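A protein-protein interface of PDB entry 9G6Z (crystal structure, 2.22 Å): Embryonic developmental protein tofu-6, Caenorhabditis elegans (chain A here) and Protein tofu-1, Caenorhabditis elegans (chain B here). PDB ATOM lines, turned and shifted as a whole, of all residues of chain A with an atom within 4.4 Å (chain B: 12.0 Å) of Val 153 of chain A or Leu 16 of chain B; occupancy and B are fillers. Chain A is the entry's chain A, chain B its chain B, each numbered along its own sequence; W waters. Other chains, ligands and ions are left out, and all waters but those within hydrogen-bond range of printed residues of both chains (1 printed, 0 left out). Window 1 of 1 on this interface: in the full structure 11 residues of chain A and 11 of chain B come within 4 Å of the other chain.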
ATOM      1  N   ASN A 149     -26.494 -19.448 -12.795  1.00  0.00           N
ATOM      2  CA  ASN A 149     -26.389 -18.937 -14.161  1.00  0.00           C
ATOM      3  C   ASN A 149     -26.980 -17.538 -14.276  1.00  0.00           C
ATOM      4  O   ASN A 149     -26.427 -16.672 -14.974  1.00  0.00           O
ATOM      5  CB  ASN A 149     -27.089 -19.882 -15.141  1.00  0.00           C
ATOM      6  CG  ASN A 149     -26.415 -21.234 -15.229  1.00  0.00           C
ATOM      7  OD1 ASN A 149     -25.302 -21.420 -14.741  1.00  0.00           O
ATOM      8  ND2 ASN A 149     -27.088 -22.186 -15.865  1.00  0.00           N
ATOM      9  N   ILE A 150     -28.112 -17.296 -13.611  1.00  0.00           N
ATOM     10  CA  ILE A 150     -28.729 -15.975 -13.691  1.00  0.00           C
ATOM     11  C   ILE A 150     -27.832 -14.927 -13.045  1.00  0.00           C
ATOM     12  O   ILE A 150     -27.714 -13.799 -13.544  1.00  0.00           O
ATOM     13  CB  ILE A 150     -30.120 -15.989 -13.044  1.00  0.00           C
ATOM     14  CG1 ILE A 150     -31.046 -16.932 -13.817  1.00  0.00           C
ATOM     15  CG2 ILE A 150     -30.712 -14.588 -13.016  1.00  0.00           C
ATOM     16  CD1 ILE A 150     -32.150 -17.528 -12.968  1.00  0.00           C
ATOM     17  N   ARG A 151     -27.165 -15.289 -11.943  1.00  0.00           N
ATOM     18  CA  ARG A 151     -26.249 -14.353 -11.301  1.00  0.00           C
ATOM     19  C   ARG A 151     -25.088 -13.993 -12.220  1.00  0.00           C
ATOM     20  O   ARG A 151     -24.662 -12.835 -12.262  1.00  0.00           O
ATOM     21  CB  ARG A 151     -25.729 -14.929  -9.982  1.00  0.00           C
ATOM     22  CG  ARG A 151     -26.545 -14.470  -8.767  1.00  0.00           C
ATOM     23  CD  ARG A 151     -25.906 -14.868  -7.430  1.00  0.00           C
ATOM     24  NE  ARG A 151     -25.965 -16.313  -7.206  1.00  0.00           N
ATOM     25  CZ  ARG A 151     -27.026 -16.961  -6.744  1.00  0.00           C
ATOM     26  NH1 ARG A 151     -28.149 -16.324  -6.416  1.00  0.00           N
ATOM     27  NH2 ARG A 151     -26.969 -18.288  -6.610  1.00  0.00           N
ATOM     28  N   GLU A 152     -24.558 -14.972 -12.960  1.00  0.00           N
ATOM     29  CA  GLU A 152     -23.477 -14.671 -13.893  1.00  0.00           C
ATOM     30  C   GLU A 152     -23.930 -13.655 -14.942  1.00  0.00           C
ATOM     31  O   GLU A 152     -23.223 -12.686 -15.241  1.00  0.00           O
ATOM     32  CB  GLU A 152     -22.978 -15.941 -14.580  1.00  0.00           C
ATOM     33  CG  GLU A 152     -22.380 -17.008 -13.666  1.00  0.00           C
ATOM     34  CD  GLU A 152     -21.890 -16.454 -12.334  1.00  0.00           C
ATOM     35  OE1 GLU A 152     -22.351 -16.963 -11.276  1.00  0.00           O
ATOM     36  OE2 GLU A 152     -21.047 -15.521 -12.338  1.00  0.00           O
ATOM     37  N   VAL A 153     -25.108 -13.884 -15.524  1.00  0.00           N
ATOM     38  CA  VAL A 153     -25.678 -12.945 -16.486  1.00  0.00           C
ATOM     39  C   VAL A 153     -25.807 -11.555 -15.870  1.00  0.00           C
ATOM     40  O   VAL A 153     -25.413 -10.549 -16.475  1.00  0.00           O
ATOM     41  CB  VAL A 153     -27.032 -13.480 -16.991  1.00  0.00           C
ATOM     42  CG1 VAL A 153     -27.984 -12.353 -17.335  1.00  0.00           C
ATOM     43  CG2 VAL A 153     -26.817 -14.395 -18.189  1.00  0.00           C
ATOM     44  N   VAL A 154     -26.349 -11.482 -14.653  1.00  0.00           N
ATOM     45  CA  VAL A 154     -26.576 -10.195 -14.009  1.00  0.00           C
ATOM     46  C   VAL A 154     -25.248  -9.497 -13.740  1.00  0.00           C
ATOM     47  O   VAL A 154     -25.150  -8.267 -13.834  1.00  0.00           O
ATOM     48  CB  VAL A 154     -27.388 -10.382 -12.713  1.00  0.00           C
ATOM     49  CG1 VAL A 154     -27.548  -9.045 -11.997  1.00  0.00           C
ATOM     50  CG2 VAL A 154     -28.753 -10.963 -13.019  1.00  0.00           C
ATOM     51  N   LYS A 155     -24.203 -10.277 -13.416  1.00  0.00           N
ATOM     52  CA  LYS A 155     -22.884  -9.689 -13.171  1.00  0.00           C
ATOM     53  C   LYS A 155     -22.329  -8.991 -14.411  1.00  0.00           C
ATOM     54  O   LYS A 155     -21.491  -8.090 -14.303  1.00  0.00           O
ATOM     55  CB  LYS A 155     -21.901 -10.768 -12.708  1.00  0.00           C
ATOM     56  CG  LYS A 155     -21.547 -10.692 -11.229  1.00  0.00           C
ATOM     57  CD  LYS A 155     -20.729 -11.895 -10.751  1.00  0.00           C
ATOM     58  CE  LYS A 155     -19.415 -12.010 -11.488  1.00  0.00           C
ATOM     59  NZ  LYS A 155     -18.560 -10.806 -11.298  1.00  0.00           N
ATOM     60  N   LYS A 156     -22.746  -9.418 -15.604  1.00  0.00           N
ATOM     61  CA  LYS A 156     -22.244  -8.825 -16.843  1.00  0.00           C
ATOM     62  C   LYS A 156     -23.234  -7.842 -17.472  1.00  0.00           C
ATOM     63  O   LYS A 156     -22.937  -7.252 -18.515  1.00  0.00           O
ATOM     64  CB  LYS A 156     -21.903  -9.906 -17.882  1.00  0.00           C
ATOM     65  CG  LYS A 156     -21.298 -11.221 -17.360  1.00  0.00           C
ATOM     66  CD  LYS A 156     -20.317 -11.072 -16.180  1.00  0.00           C
ATOM     67  CE  LYS A 156     -19.266  -9.974 -16.368  1.00  0.00           C
ATOM     68  NZ  LYS A 156     -18.280 -10.000 -15.224  1.00  0.00           N
ATOM     69  N   TRP A 157     -24.402  -7.669 -16.863  1.00  0.00           N
ATOM     70  CA  TRP A 157     -25.462  -6.858 -17.456  1.00  0.00           C
ATOM     71  C   TRP A 157     -25.029  -5.409 -17.634  1.00  0.00           C
ATOM     72  O   TRP A 157     -25.256  -4.813 -18.693  1.00  0.00           O
ATOM     73  CB  TRP A 157     -26.707  -6.960 -16.566  1.00  0.00           C
ATOM     74  CG  TRP A 157     -27.855  -6.098 -16.940  1.00  0.00           C
ATOM     75  CD1 TRP A 157     -28.098  -5.513 -18.148  1.00  0.00           C
ATOM     76  CD2 TRP A 157     -28.935  -5.719 -16.083  1.00  0.00           C
ATOM     77  NE1 TRP A 157     -29.264  -4.792 -18.095  1.00  0.00           N
ATOM     78  CE2 TRP A 157     -29.799  -4.904 -16.838  1.00  0.00           C
ATOM     79  CE3 TRP A 157     -29.257  -6.000 -14.757  1.00  0.00           C
ATOM     80  CZ2 TRP A 157     -30.964  -4.364 -16.313  1.00  0.00           C
ATOM     81  CZ3 TRP A 157     -30.425  -5.464 -14.228  1.00  0.00           C
ATOM     82  CH2 TRP A 157     -31.262  -4.652 -15.010  1.00  0.00           C
ATOM     83  N   ARG A 191     -38.046  -8.346 -16.432  1.00  0.00           N
ATOM     84  CA  ARG A 191     -37.553  -9.173 -17.535  1.00  0.00           C
ATOM     85  C   ARG A 191     -37.561 -10.655 -17.171  1.00  0.00           C
ATOM     86  O   ARG A 191     -37.762 -11.507 -18.043  1.00  0.00           O
ATOM     87  CB  ARG A 191     -36.143  -8.734 -17.929  1.00  0.00           C
ATOM     88  CG  ARG A 191     -36.018  -7.253 -18.282  1.00  0.00           C
ATOM     89  CD  ARG A 191     -36.542  -6.967 -19.685  1.00  0.00           C
ATOM     90  NE  ARG A 191     -37.936  -6.526 -19.695  1.00  0.00           N
ATOM     91  CZ  ARG A 191     -38.694  -6.497 -20.782  1.00  0.00           C
ATOM     92  NH1 ARG A 191     -38.253  -6.957 -21.941  1.00  0.00           N
ATOM     93  NH2 ARG A 191     -39.923  -5.997 -20.702  1.00  0.00           N
ATOM     94  N   LEU A 192     -37.331 -10.983 -15.898  1.00  0.00           N
ATOM     95  CA  LEU A 192     -37.440 -12.369 -15.460  1.00  0.00           C
ATOM     96  C   LEU A 192     -38.892 -12.829 -15.471  1.00  0.00           C
ATOM     97  O   LEU A 192     -39.229 -13.853 -16.069  1.00  0.00           O
ATOM     98  CB  LEU A 192     -36.845 -12.519 -14.064  1.00  0.00           C
ATOM     99  CG  LEU A 192     -35.332 -12.406 -13.936  1.00  0.00           C
ATOM    100  CD1 LEU A 192     -34.958 -12.090 -12.496  1.00  0.00           C
ATOM    101  CD2 LEU A 192     -34.653 -13.690 -14.395  1.00  0.00           C
ATOM    102  N   LYS A 195     -40.202 -13.918 -18.668  1.00  0.00           N
ATOM    103  CA  LYS A 195     -39.804 -15.236 -19.136  1.00  0.00           C
ATOM    104  C   LYS A 195     -40.561 -16.366 -18.454  1.00  0.00           C
ATOM    105  O   LYS A 195     -40.276 -17.535 -18.724  1.00  0.00           O
ATOM    106  CB  LYS A 195     -38.297 -15.432 -18.936  1.00  0.00           C
ATOM    107  CG  LYS A 195     -37.458 -14.477 -19.782  1.00  0.00           C
ATOM    108  CD  LYS A 195     -36.046 -14.990 -19.971  1.00  0.00           C
ATOM    109  CE  LYS A 195     -35.247 -14.051 -20.871  1.00  0.00           C
ATOM    110  NZ  LYS A 195     -35.789 -13.997 -22.260  1.00  0.00           N
ATOM    111  N   GLU B   9     -37.480  -7.521 -27.952  1.00  0.00           N
ATOM    112  CA  GLU B   9     -36.647  -8.296 -27.034  1.00  0.00           C
ATOM    113  C   GLU B   9     -35.424  -7.473 -26.615  1.00  0.00           C
ATOM    114  O   GLU B   9     -34.556  -7.166 -27.430  1.00  0.00           O
ATOM    115  CB  GLU B   9     -36.220  -9.609 -27.687  1.00  0.00           C
ATOM    116  CG  GLU B   9     -35.365 -10.510 -26.801  1.00  0.00           C
ATOM    117  CD  GLU B   9     -36.117 -11.733 -26.286  1.00  0.00           C
ATOM    118  OE1 GLU B   9     -37.368 -11.707 -26.248  1.00  0.00           O
ATOM    119  OE2 GLU B   9     -35.451 -12.725 -25.918  1.00  0.00           O
ATOM    120  N   SER B  10     -35.363  -7.131 -25.332  1.00  0.00           N
ATOM    121  CA  SER B  10     -34.327  -6.250 -24.826  1.00  0.00           C
ATOM    122  C   SER B  10     -32.961  -6.938 -24.875  1.00  0.00           C
ATOM    123  O   SER B  10     -32.822  -8.109 -25.243  1.00  0.00           O
ATOM    124  CB  SER B  10     -34.639  -5.826 -23.386  1.00  0.00           C
ATOM    125  OG  SER B  10     -34.383  -6.896 -22.489  1.00  0.00           O
ATOM    126  N   LEU B  11     -31.931  -6.183 -24.487  1.00  0.00           N
ATOM    127  CA  LEU B  11     -30.607  -6.771 -24.292  1.00  0.00           C
ATOM    128  C   LEU B  11     -30.630  -7.792 -23.162  1.00  0.00           C
ATOM    129  O   LEU B  11     -30.161  -8.926 -23.319  1.00  0.00           O
ATOM    130  CB  LEU B  11     -29.592  -5.663 -24.001  1.00  0.00           C
ATOM    131  CG  LEU B  11     -28.118  -5.992 -23.817  1.00  0.00           C
ATOM    132  CD1 LEU B  11     -27.332  -4.666 -23.723  1.00  0.00           C
ATOM    133  CD2 LEU B  11     -27.835  -6.841 -22.599  1.00  0.00           C
ATOM    134  N   LEU B  12     -31.153  -7.394 -21.998  1.00  0.00           N
ATOM    135  CA  LEU B  12     -31.144  -8.288 -20.841  1.00  0.00           C
ATOM    136  C   LEU B  12     -31.919  -9.573 -21.120  1.00  0.00           C
ATOM    137  O   LEU B  12     -31.540 -10.654 -20.646  1.00  0.00           O
ATOM    138  CB  LEU B  12     -31.721  -7.566 -19.626  1.00  0.00           C
ATOM    139  CG  LEU B  12     -31.720  -8.344 -18.307  1.00  0.00           C
ATOM    140  CD1 LEU B  12     -30.298  -8.654 -17.863  1.00  0.00           C
ATOM    141  CD2 LEU B  12     -32.457  -7.564 -17.219  1.00  0.00           C
ATOM    142  N   ASP B  13     -33.006  -9.471 -21.886  1.00  0.00           N
ATOM    143  CA  ASP B  13     -33.716 -10.659 -22.343  1.00  0.00           C
ATOM    144  C   ASP B  13     -32.749 -11.698 -22.890  1.00  0.00           C
ATOM    145  O   ASP B  13     -32.722 -12.852 -22.445  1.00  0.00           O
ATOM    146  CB  ASP B  13     -34.737 -10.285 -23.424  1.00  0.00           C
ATOM    147  CG  ASP B  13     -35.810  -9.364 -22.904  1.00  0.00           C
ATOM    148  OD1 ASP B  13     -35.766  -9.044 -21.707  1.00  0.00           O
ATOM    149  OD2 ASP B  13     -36.699  -8.966 -23.692  1.00  0.00           O
ATOM    150  N   ALA B  14     -31.951 -11.294 -23.878  1.00  0.00           N
ATOM    151  CA  ALA B  14     -31.009 -12.212 -24.506  1.00  0.00           C
ATOM    152  C   ALA B  14     -30.075 -12.828 -23.475  1.00  0.00           C
ATOM    153  O   ALA B  14     -29.851 -14.044 -23.469  1.00  0.00           O
ATOM    154  CB  ALA B  14     -30.206 -11.479 -25.586  1.00  0.00           C
ATOM    155  N   LEU B  15     -29.519 -12.000 -22.592  1.00  0.00           N
ATOM    156  CA  LEU B  15     -28.673 -12.525 -21.525  1.00  0.00           C
ATOM    157  C   LEU B  15     -29.411 -13.584 -20.713  1.00  0.00           C
ATOM    158  O   LEU B  15     -28.915 -14.698 -20.515  1.00  0.00           O
ATOM    159  CB  LEU B  15     -28.214 -11.389 -20.610  1.00  0.00           C
ATOM    160  CG  LEU B  15     -27.662 -10.109 -21.232  1.00  0.00           C
ATOM    161  CD1 LEU B  15     -27.365  -9.082 -20.129  1.00  0.00           C
ATOM    162  CD2 LEU B  15     -26.414 -10.366 -22.047  1.00  0.00           C
ATOM    163  N   LEU B  16     -30.611 -13.245 -20.236  1.00  0.00           N
ATOM    164  CA  LEU B  16     -31.362 -14.179 -19.408  1.00  0.00           C
ATOM    165  C   LEU B  16     -31.749 -15.430 -20.185  1.00  0.00           C
ATOM    166  O   LEU B  16     -31.787 -16.528 -19.617  1.00  0.00           O
ATOM    167  CB  LEU B  16     -32.613 -13.502 -18.844  1.00  0.00           C
ATOM    168  CG  LEU B  16     -32.366 -12.380 -17.835  1.00  0.00           C
ATOM    169  CD1 LEU B  16     -33.674 -11.648 -17.569  1.00  0.00           C
ATOM    170  CD2 LEU B  16     -31.776 -12.926 -16.550  1.00  0.00           C
ATOM    171  N   GLY B  17     -32.035 -15.282 -21.475  1.00  0.00           N
ATOM    172  CA  GLY B  17     -32.382 -16.442 -22.278  1.00  0.00           C
ATOM    173  C   GLY B  17     -31.294 -17.496 -22.311  1.00  0.00           C
ATOM    174  O   GLY B  17     -31.576 -18.695 -22.244  1.00  0.00           O
ATOM    175  N   LYS B  18     -30.036 -17.068 -22.399  1.00  0.00           N
ATOM    176  CA  LYS B  18     -28.947 -18.037 -22.422  1.00  0.00           C
ATOM    177  C   LYS B  18     -28.780 -18.708 -21.063  1.00  0.00           C
ATOM    178  O   LYS B  18     -28.587 -19.927 -20.989  1.00  0.00           O
ATOM    179  CB  LYS B  18     -27.635 -17.375 -22.867  1.00  0.00           C
ATOM    180  CG  LYS B  18     -27.110 -16.266 -21.968  1.00  0.00           C
ATOM    181  CD  LYS B  18     -25.576 -16.233 -21.942  1.00  0.00           C
ATOM    182  CE  LYS B  18     -25.032 -16.941 -20.706  1.00  0.00           C
ATOM    183  NZ  LYS B  18     -23.616 -16.562 -20.419  1.00  0.00           N
ATOM    184  N   ALA B  19     -28.887 -17.938 -19.979  1.00  0.00           N
ATOM    185  CA  ALA B  19     -28.783 -18.528 -18.648  1.00  0.00           C
ATOM    186  C   ALA B  19     -29.833 -19.610 -18.422  1.00  0.00           C
ATOM    187  O   ALA B  19     -29.579 -20.585 -17.703  1.00  0.00           O
ATOM    188  CB  ALA B  19     -28.924 -17.437 -17.575  1.00  0.00           C
ATOM    189  N   LEU B  20     -31.011 -19.452 -19.013  1.00  0.00           N
ATOM    190  CA  LEU B  20     -32.122 -20.367 -18.778  1.00  0.00           C
ATOM    191  C   LEU B  20     -32.134 -21.497 -19.802  1.00  0.00           C
ATOM    192  O   LEU B  20     -32.590 -22.600 -19.516  1.00  0.00           O
ATOM    193  CB  LEU B  20     -33.445 -19.599 -18.817  1.00  0.00           C
ATOM    194  CG  LEU B  20     -33.588 -18.492 -17.773  1.00  0.00           C
ATOM    195  CD1 LEU B  20     -34.735 -17.550 -18.118  1.00  0.00           C
ATOM    196  CD2 LEU B  20     -33.789 -19.087 -16.385  1.00  0.00           C
HETATM  197  O   HOH W   1     -37.278 -11.277 -20.870  1.00  0.00           O
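Water W1 lies within hydrogen-bond range of the side-chain carboxylate of Asp 13 of chain B, the backbone carbonyl oxygen of Arg 191 of chain A and the side-chain amino group of Lys 195 of chain A.
Of the 12 printed residues of chain B, 9 touch a printed residue of chain A. Printed residues of chain B that touch a printed residue of chain A: Glu 9, Ser 10, Leu 12, Asp 13, Leu 15, Leu 16, Gly 17, Ala 19 and Leu 20. Of the 12 printed residues of chain A, 6 touch a printed residue of chain B. Printed residues of chain A that touch a printed residue of chain B: Asn 149, Val 153, Trp 157, Arg 191, Leu 192 and Lys 195. Hydrophobic or aromatic side chains of chain A within 4 Å of the printed part of chain B: Val 153, Trp 157 and Leu 192. Among the printed residues, 16 pairs touch across the chains. Among the printed residues, Asp or Glu carboxylates within 4 Å of a Lys or Arg side-chain nitrogen of the other chain: Arg 191 of chain A with Asp 13 of chain B (3.1 Å) and Lys 195 of chain A with Glu 9 of chain B (3.9 Å).
The side-chain amide nitrogen of Asn 149 of chain A is in hydrogen-bond range of the backbone carbonyl oxygen of Ala 19 of chain B, 3.5 Å away. The side-chain amino group (NZ) of Lys 195 of chain A lies within salt-bridge range of the side-chain carboxylate (OE2) of Glu 9 of chain B (3.9 Å). The side-chain amino group (NZ) of Lys 195 of chain A sits close to the backbone carbonyl oxygen (O) of Asp 13 of chain B, at 3.3 Å. The guanidinium group (NH1) of Arg 191 of chain A lies within salt-bridge range of the side-chain carboxylate (OD2) of Asp 13 of chain B, 3.1 Å away.
Val 153 of chain A touches Leu 15 of chain B (CG2 to O, 3.1 Å). CG1 of Val 153 of chain A touches CD2 of Leu 16 of chain B, 3.9 Å away. Ala 19 of chain B touches Val 153 of chain A. Trp 157 of chain A touches Leu 12 of chain B. CD1 of Leu 15 of chain B touches CA of Trp 157 of chain A, at 3.96 Å. OG of Ser 10 of chain B touches CD of Arg 191 of chain A, at 3.5 Å. CB of Arg 191 of chain A touches CD1 of Leu 16 of chain B, at 3.8 Å. CE of Lys 195 of chain A touches CB of Leu 16 of chain B, at 3.4 Å. Gly 17 of chain B touches Lys 195 of chain A. CD1 of Leu 20 of chain B touches CD of Lys 195 of chain A (3.4 Å).
Arg 151 of chain A touches none of the printed residues of chain B. Of the printed residues of chain B, Val 153 of chain A touches Leu 15 (3.1 Å), Leu 16 (3.9 Å) and Ala 19 (3.8 Å). No residue of chain B comes within 4 Å of Val 154 of chain A. No residue of chain B comes within 4 Å of Lys 156 of chain A. Trp 157 of chain A touches just these residues of chain B: Leu 12 and Leu 15. Leu 192 of chain A touches just one residue of chain B: Leu 16. Of the printed residues of chain B, Lys 195 of chain A touches Glu 9, Asp 13, Leu 16, Gly 17 and Leu 20. Leu 11 of chain B touches none of the printed residues of chain A. Printed residues of chain A within 4 Å of Leu 15 of chain B: Val 153 and Trp 157. Of chain A, only Val 153, Arg 191, Leu 192 and Lys 195 come within 4 Å of Leu 16 of chain B. Printed residues of chain A within 4 Å of Gly 17 of chain B: Lys 195 (3.5 Å). The nearest printed residue of chain B that does not touch Val 153 of chain A is Lys 18 of chain B (4.0005 Å). The nearest printed residue of chain A that does not touch Glu 9 of chain B is Arg 191 of chain A (5.5 Å).
The backbone NH (N) of Leu 12 of chain B is in hydrogen-bond range of the side-chain hydroxyl (OG) of Ser 10 of chain B (3.3 Å). The side-chain hydroxyl of Ser 10 of chain B is in hydrogen-bond range of the side-chain carboxylate of Asp 13 of chain B.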
